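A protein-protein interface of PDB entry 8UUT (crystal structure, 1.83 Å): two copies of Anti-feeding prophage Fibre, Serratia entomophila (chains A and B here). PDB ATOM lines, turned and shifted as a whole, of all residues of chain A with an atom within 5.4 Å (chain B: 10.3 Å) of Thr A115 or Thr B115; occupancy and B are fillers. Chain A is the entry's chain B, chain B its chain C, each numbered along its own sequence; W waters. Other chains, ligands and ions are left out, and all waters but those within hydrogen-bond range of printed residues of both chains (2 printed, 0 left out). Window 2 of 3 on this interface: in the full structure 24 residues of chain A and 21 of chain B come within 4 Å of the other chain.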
ATOM      1  N   ILE A 111       6.887  -0.781  28.012  1.00  0.00           N
ATOM      2  CA  ILE A 111       5.457  -0.654  28.282  1.00  0.00           C
ATOM      3  C   ILE A 111       4.773  -0.384  26.948  1.00  0.00           C
ATOM      4  O   ILE A 111       5.108   0.603  26.269  1.00  0.00           O
ATOM      5  CB  ILE A 111       5.142   0.485  29.267  1.00  0.00           C
ATOM      6  CG1 ILE A 111       5.626   0.155  30.680  1.00  0.00           C
ATOM      7  CG2 ILE A 111       3.651   0.793  29.302  1.00  0.00           C
ATOM      8  CD1 ILE A 111       5.549   1.359  31.606  1.00  0.00           C
ATOM      9  N   LEU A 112       3.827  -1.244  26.565  1.00  0.00           N
ATOM     10  CA  LEU A 112       2.945  -0.927  25.446  1.00  0.00           C
ATOM     11  C   LEU A 112       1.600  -0.439  25.975  1.00  0.00           C
ATOM     12  O   LEU A 112       1.169  -0.804  27.077  1.00  0.00           O
ATOM     13  CB  LEU A 112       2.741  -2.125  24.509  1.00  0.00           C
ATOM     14  CG  LEU A 112       3.999  -2.809  23.953  1.00  0.00           C
ATOM     15  CD1 LEU A 112       3.634  -3.943  22.979  1.00  0.00           C
ATOM     16  CD2 LEU A 112       4.957  -1.806  23.284  1.00  0.00           C
ATOM     17  N   ALA A 113       0.945   0.409  25.189  1.00  0.00           N
ATOM     18  CA  ALA A 113      -0.214   1.131  25.694  1.00  0.00           C
ATOM     19  C   ALA A 113      -1.284   1.296  24.629  1.00  0.00           C
ATOM     20  O   ALA A 113      -1.021   1.228  23.431  1.00  0.00           O
ATOM     21  CB  ALA A 113       0.172   2.526  26.213  1.00  0.00           C
ATOM     22  N   MET A 114      -2.508   1.453  25.116  1.00  0.00           N
ATOM     23  CA  MET A 114      -3.602   2.102  24.421  1.00  0.00           C
ATOM     24  C   MET A 114      -3.514   3.605  24.679  1.00  0.00           C
ATOM     25  O   MET A 114      -3.235   4.033  25.801  1.00  0.00           O
ATOM     26  CB  MET A 114      -4.899   1.457  24.919  1.00  0.00           C
ATOM     27  CG  MET A 114      -5.428   2.009  26.249  1.00  0.00           C
ATOM     28  SD  MET A 114      -6.985   1.304  26.858  1.00  0.00           S
ATOM     29  CE  MET A 114      -6.672  -0.468  26.790  1.00  0.00           C
ATOM     30  N   THR A 115      -3.686   4.403  23.623  1.00  0.00           N
ATOM     31  CA  THR A 115      -3.313   5.817  23.661  1.00  0.00           C
ATOM     32  C   THR A 115      -4.458   6.702  23.187  1.00  0.00           C
ATOM     33  O   THR A 115      -5.343   6.272  22.438  1.00  0.00           O
ATOM     34  CB  THR A 115      -2.075   6.099  22.783  1.00  0.00           C
ATOM     35  OG1 THR A 115      -2.372   5.768  21.428  1.00  0.00           O
ATOM     36  CG2 THR A 115      -0.892   5.249  23.223  1.00  0.00           C
ATOM     37  N   GLY A 116      -4.417   7.959  23.626  1.00  0.00           N
ATOM     38  CA  GLY A 116      -5.363   8.970  23.187  1.00  0.00           C
ATOM     39  C   GLY A 116      -4.960  10.340  23.693  1.00  0.00           C
ATOM     40  O   GLY A 116      -4.837  10.521  24.906  1.00  0.00           O
ATOM     41  N   GLY A 117      -4.760  11.310  22.801  1.00  0.00           N
ATOM     42  CA  GLY A 117      -4.161  12.558  23.261  1.00  0.00           C
ATOM     43  C   GLY A 117      -2.844  12.268  23.953  1.00  0.00           C
ATOM     44  O   GLY A 117      -2.050  11.434  23.503  1.00  0.00           O
ATOM     45  N   SER A 119      -2.809  10.955  26.970  1.00  0.00           N
ATOM     46  CA  SER A 119      -3.118   9.919  27.946  1.00  0.00           C
ATOM     47  C   SER A 119      -2.788   8.541  27.378  1.00  0.00           C
ATOM     48  O   SER A 119      -2.831   8.321  26.161  1.00  0.00           O
ATOM     49  CB  SER A 119      -4.592   9.988  28.338  1.00  0.00           C
ATOM     50  OG  SER A 119      -4.890  11.260  28.872  1.00  0.00           O
ATOM     51  N   SER A 120      -2.464   7.606  28.269  1.00  0.00           N
ATOM     52  CA  SER A 120      -2.183   6.244  27.834  1.00  0.00           C
ATOM     53  C   SER A 120      -2.307   5.298  29.020  1.00  0.00           C
ATOM     54  O   SER A 120      -2.070   5.687  30.166  1.00  0.00           O
ATOM     55  CB  SER A 120      -0.791   6.135  27.208  1.00  0.00           C
ATOM     56  OG  SER A 120       0.190   6.610  28.104  1.00  0.00           O
ATOM     57  N   ALA A 121      -2.682   4.054  28.731  1.00  0.00           N
ATOM     58  CA  ALA A 121      -2.907   3.033  29.750  1.00  0.00           C
ATOM     59  C   ALA A 121      -2.104   1.794  29.392  1.00  0.00           C
ATOM     60  O   ALA A 121      -2.127   1.359  28.238  1.00  0.00           O
ATOM     61  CB  ALA A 121      -4.393   2.666  29.857  1.00  0.00           C
ATOM     62  N   TYR B  93       4.232 -11.686  21.397  1.00  0.00           N
ATOM     63  CA  TYR B  93       3.221 -10.913  20.685  1.00  0.00           C
ATOM     64  C   TYR B  93       3.570 -10.984  19.201  1.00  0.00           C
ATOM     65  O   TYR B  93       4.640 -11.470  18.829  1.00  0.00           O
ATOM     66  CB  TYR B  93       3.163  -9.466  21.198  1.00  0.00           C
ATOM     67  CG  TYR B  93       4.416  -8.645  20.929  1.00  0.00           C
ATOM     68  CD1 TYR B  93       4.610  -8.005  19.705  1.00  0.00           C
ATOM     69  CD2 TYR B  93       5.397  -8.498  21.905  1.00  0.00           C
ATOM     70  CE1 TYR B  93       5.740  -7.261  19.461  1.00  0.00           C
ATOM     71  CE2 TYR B  93       6.534  -7.746  21.665  1.00  0.00           C
ATOM     72  CZ  TYR B  93       6.699  -7.135  20.447  1.00  0.00           C
ATOM     73  OH  TYR B  93       7.826  -6.394  20.200  1.00  0.00           O
ATOM     74  N   LEU B  94       2.659 -10.514  18.342  1.00  0.00           N
ATOM     75  CA  LEU B  94       2.889 -10.531  16.901  1.00  0.00           C
ATOM     76  C   LEU B  94       3.461  -9.202  16.418  1.00  0.00           C
ATOM     77  O   LEU B  94       2.925  -8.133  16.729  1.00  0.00           O
ATOM     78  CB  LEU B  94       1.609 -10.860  16.120  1.00  0.00           C
ATOM     79  CG  LEU B  94       0.955 -12.226  16.360  1.00  0.00           C
ATOM     80  CD1 LEU B  94      -0.047 -12.506  15.246  1.00  0.00           C
ATOM     81  CD2 LEU B  94       1.998 -13.349  16.433  1.00  0.00           C
ATOM     82  N   THR B  96       4.292  -6.024  14.188  1.00  0.00           N
ATOM     83  CA  THR B  96       3.463  -5.148  13.377  1.00  0.00           C
ATOM     84  C   THR B  96       4.118  -4.771  12.057  1.00  0.00           C
ATOM     85  O   THR B  96       3.493  -4.070  11.258  1.00  0.00           O
ATOM     86  CB  THR B  96       3.141  -3.865  14.137  1.00  0.00           C
ATOM     87  OG1 THR B  96       4.362  -3.207  14.471  1.00  0.00           O
ATOM     88  CG2 THR B  96       2.383  -4.177  15.430  1.00  0.00           C
ATOM     89  N   ILE B 111      -3.350  -2.935  10.074  1.00  0.00           N
ATOM     90  CA  ILE B 111      -2.971  -3.460  11.385  1.00  0.00           C
ATOM     91  C   ILE B 111      -3.172  -2.343  12.403  1.00  0.00           C
ATOM     92  O   ILE B 111      -2.655  -1.240  12.212  1.00  0.00           O
ATOM     93  CB  ILE B 111      -1.499  -3.937  11.400  1.00  0.00           C
ATOM     94  CG1 ILE B 111      -1.309  -5.202  10.555  1.00  0.00           C
ATOM     95  CG2 ILE B 111      -0.982  -4.139  12.812  1.00  0.00           C
ATOM     96  CD1 ILE B 111       0.118  -5.755  10.613  1.00  0.00           C
ATOM     97  N   LEU B 112      -3.932  -2.612  13.469  1.00  0.00           N
ATOM     98  CA  LEU B 112      -3.973  -1.733  14.635  1.00  0.00           C
ATOM     99  C   LEU B 112      -3.142  -2.357  15.752  1.00  0.00           C
ATOM    100  O   LEU B 112      -3.023  -3.581  15.849  1.00  0.00           O
ATOM    101  CB  LEU B 112      -5.413  -1.504  15.123  1.00  0.00           C
ATOM    102  CG  LEU B 112      -6.505  -1.096  14.119  1.00  0.00           C
ATOM    103  CD1 LEU B 112      -7.777  -0.728  14.859  1.00  0.00           C
ATOM    104  CD2 LEU B 112      -6.054   0.076  13.255  1.00  0.00           C
ATOM    105  N   ALA B 113      -2.548  -1.518  16.595  1.00  0.00           N
ATOM    106  CA  ALA B 113      -1.602  -2.041  17.566  1.00  0.00           C
ATOM    107  C   ALA B 113      -1.706  -1.304  18.894  1.00  0.00           C
ATOM    108  O   ALA B 113      -2.223  -0.188  18.974  1.00  0.00           O
ATOM    109  CB  ALA B 113      -0.158  -1.933  17.045  1.00  0.00           C
ATOM    110  N   MET B 114      -1.221  -1.964  19.945  1.00  0.00           N
ATOM    111  CA  MET B 114      -0.790  -1.261  21.142  1.00  0.00           C
ATOM    112  C   MET B 114       0.666  -0.855  20.940  1.00  0.00           C
ATOM    113  O   MET B 114       1.443  -1.592  20.326  1.00  0.00           O
ATOM    114  CB  MET B 114      -0.894  -2.099  22.416  1.00  0.00           C
ATOM    115  CG  MET B 114      -0.127  -3.415  22.371  1.00  0.00           C
ATOM    116  SD  MET B 114      -0.393  -4.532  23.777  1.00  0.00           S
ATOM    117  CE  MET B 114      -2.067  -5.123  23.671  1.00  0.00           C
ATOM    118  N   THR B 115       1.040   0.320  21.458  1.00  0.00           N
ATOM    119  CA  THR B 115       2.289   0.942  21.037  1.00  0.00           C
ATOM    120  C   THR B 115       3.130   1.400  22.220  1.00  0.00           C
ATOM    121  O   THR B 115       2.617   1.748  23.289  1.00  0.00           O
ATOM    122  CB  THR B 115       2.030   2.141  20.116  1.00  0.00           C
ATOM    123  OG1 THR B 115       1.331   3.158  20.843  1.00  0.00           O
ATOM    124  CG2 THR B 115       1.192   1.726  18.890  1.00  0.00           C
ATOM    125  N   GLY B 116       4.444   1.411  22.000  1.00  0.00           N
ATOM    126  CA  GLY B 116       5.387   1.867  23.000  1.00  0.00           C
ATOM    127  C   GLY B 116       6.537   2.601  22.338  1.00  0.00           C
ATOM    128  O   GLY B 116       6.560   2.779  21.117  1.00  0.00           O
ATOM    129  N   GLY B 117       7.491   3.026  23.166  1.00  0.00           N
ATOM    130  CA  GLY B 117       8.608   3.799  22.653  1.00  0.00           C
ATOM    131  C   GLY B 117       9.492   3.045  21.678  1.00  0.00           C
ATOM    132  O   GLY B 117      10.088   3.656  20.787  1.00  0.00           O
ATOM    133  N   SER B 118       9.582   1.717  21.815  1.00  0.00           N
ATOM    134  CA  SER B 118      10.472   0.915  20.987  1.00  0.00           C
ATOM    135  C   SER B 118       9.785  -0.210  20.236  1.00  0.00           C
ATOM    136  O   SER B 118      10.400  -0.779  19.325  1.00  0.00           O
ATOM    137  CB  SER B 118      11.596   0.299  21.839  1.00  0.00           C
ATOM    138  OG  SER B 118      12.338   1.293  22.527  1.00  0.00           O
ATOM    139  N   SER B 119       8.551  -0.567  20.596  1.00  0.00           N
ATOM    140  CA  SER B 119       7.888  -1.733  20.029  1.00  0.00           C
ATOM    141  C   SER B 119       6.408  -1.433  19.849  1.00  0.00           C
ATOM    142  O   SER B 119       5.882  -0.435  20.342  1.00  0.00           O
ATOM    143  CB  SER B 119       8.050  -2.971  20.926  1.00  0.00           C
ATOM    144  OG  SER B 119       9.412  -3.226  21.205  1.00  0.00           O
ATOM    145  N   SER B 120       5.728  -2.338  19.153  1.00  0.00           N
ATOM    146  CA  SER B 120       4.282  -2.277  19.008  1.00  0.00           C
ATOM    147  C   SER B 120       3.813  -3.690  18.704  1.00  0.00           C
ATOM    148  O   SER B 120       4.545  -4.470  18.088  1.00  0.00           O
ATOM    149  CB  SER B 120       3.871  -1.287  17.917  1.00  0.00           C
ATOM    150  OG  SER B 120       4.447  -1.630  16.673  1.00  0.00           O
ATOM    151  N   ALA B 121       2.606  -4.027  19.170  1.00  0.00           N
ATOM    152  CA  ALA B 121       2.088  -5.387  19.066  1.00  0.00           C
ATOM    153  C   ALA B 121       0.725  -5.365  18.391  1.00  0.00           C
ATOM    154  O   ALA B 121      -0.110  -4.522  18.711  1.00  0.00           O
ATOM    155  CB  ALA B 121       1.957  -6.042  20.452  1.00  0.00           C
ATOM    156  N   VAL B 122       0.500  -6.308  17.473  1.00  0.00           N
ATOM    157  CA  VAL B 122      -0.773  -6.360  16.758  1.00  0.00           C
ATOM    158  C   VAL B 122      -1.917  -6.628  17.721  1.00  0.00           C
ATOM    159  O   VAL B 122      -1.857  -7.550  18.543  1.00  0.00           O
ATOM    160  CB  VAL B 122      -0.743  -7.450  15.678  1.00  0.00           C
ATOM    161  CG1 VAL B 122      -2.130  -7.577  15.043  1.00  0.00           C
ATOM    162  CG2 VAL B 122       0.328  -7.158  14.632  1.00  0.00           C
ATOM    163  N   THR B 123      -2.981  -5.835  17.605  1.00  0.00           N
ATOM    164  CA  THR B 123      -4.233  -6.112  18.297  1.00  0.00           C
ATOM    165  C   THR B 123      -5.397  -6.365  17.352  1.00  0.00           C
ATOM    166  O   THR B 123      -6.399  -6.960  17.769  1.00  0.00           O
ATOM    167  CB  THR B 123      -4.606  -4.948  19.227  1.00  0.00           C
ATOM    168  OG1 THR B 123      -4.557  -3.725  18.492  1.00  0.00           O
ATOM    169  CG2 THR B 123      -3.591  -4.852  20.372  1.00  0.00           C
ATOM    170  N   LEU B 145       8.813  -8.570  24.378  1.00  0.00           N
ATOM    171  CA  LEU B 145       9.338  -7.337  24.932  1.00  0.00           C
ATOM    172  C   LEU B 145      10.561  -7.588  25.793  1.00  0.00           C
ATOM    173  O   LEU B 145      11.298  -6.644  26.084  1.00  0.00           O
ATOM    174  CB  LEU B 145       8.278  -6.624  25.771  1.00  0.00           C
ATOM    175  CG  LEU B 145       7.021  -6.092  25.084  1.00  0.00           C
ATOM    176  CD1 LEU B 145       6.066  -5.466  26.080  1.00  0.00           C
ATOM    177  CD2 LEU B 145       7.407  -5.093  24.012  1.00  0.00           C
HETATM  178  O   HOH W   1       8.408   1.396  26.116  1.00  0.00           O
HETATM  179  O   HOH W   2      -1.669   3.377  20.430  1.00  0.00           O
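The backbone NH (N) of Ala A113 sits at hydrogen-bond distance from the backbone carbonyl oxygen (O) of Thr B115 (2.9 Å).
O of Met B114 lies within hydrogen-bond range of N of Ala B121, 2.9 Å away.
Ile A111 touches Gly B116 (O to CA, 3.5 Å).
CB of Leu A112 touches CG of Met B114, 3.8 Å away.
Leu A112 touches Thr B115.
Leu A112 touches Gly B116.
Leu A112 touches Ser B119.
Ala B121 touches Leu A112 (CB to CD1, 3.7 Å).
Leu B145 touches Leu A112.
Met B114 touches Ala A113 (CA to O, 3.4 Å).
Thr B115 touches Thr A115 (OG1 to CG2, 3.9 Å).
Of chain B, only Met B114 (3.4 Å) and Thr B115 (2.9 Å) come within 4 Å of Ala A113.
No residue of chain B comes within 4 Å of Gly A116.
Gly A117 touches none of the printed residues of chain B.
Printed residues of chain A within 4 Å of Ser B119: Leu A112.
Of the printed residues of chain A, Met B114 touches Leu A112 and Ala A113.
Printed residues of chain B within 4 Å of Ile A111: Gly B116.
Of the printed residues of chain A, Ala B121 touches Leu A112.
Printed residues of chain B within 4 Å of Leu A112: Met B114 (3.8 Å), Thr B115 (3.5 Å), Gly B116 (3.5 Å), Ser B119 (3.4 Å), Ala B121 (3.7 Å) and Leu B145 (3.98 Å).
Gly B117 touches none of the printed residues of chain A.
Tyr B93 touches none of the printed residues of chain A.
The nearest residue of chain B that does not touch Thr A115 is Ala B113 (6.4 Å).
Of the 10 printed residues of chain A, 4 touch a printed residue of chain B.
Printed residues of chain A that touch a printed residue of chain B: Ile A111, Leu A112, Ala A113 and Thr A115.
Along chain B the printed residues that touch a printed residue of chain A span positions 114 to 145.
Among the printed residues, 10 pairs touch across the chains.
Among the printed residues, no Asp or Glu carboxylate lies within 4 Å of a Lys or Arg side-chain nitrogen of the other chain.
Ile A111 touches Gly B116, but with the chains exchanged Gly A116 does not touch Ile B111 (14.8 Å).
Leu A112 touches Ser B119, but with the chains exchanged Ser A119 does not touch Leu B112 (14.9 Å).
Leu A112 touches Ala B121, but with the chains exchanged Ala A121 does not touch Leu B112 (13.1 Å).
Thr A115 touches its own counterpart, Thr B115.
10 positions are printed for both chains.
Water W2 lies within hydrogen-bond range of the side-chain hydroxyl of Thr A115 (2.7 Å) and the side-chain hydroxyl of Thr B115 (3.0 Å).
Water W1 lies within hydrogen-bond range of N of Ile A111 and N of Gly B117.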
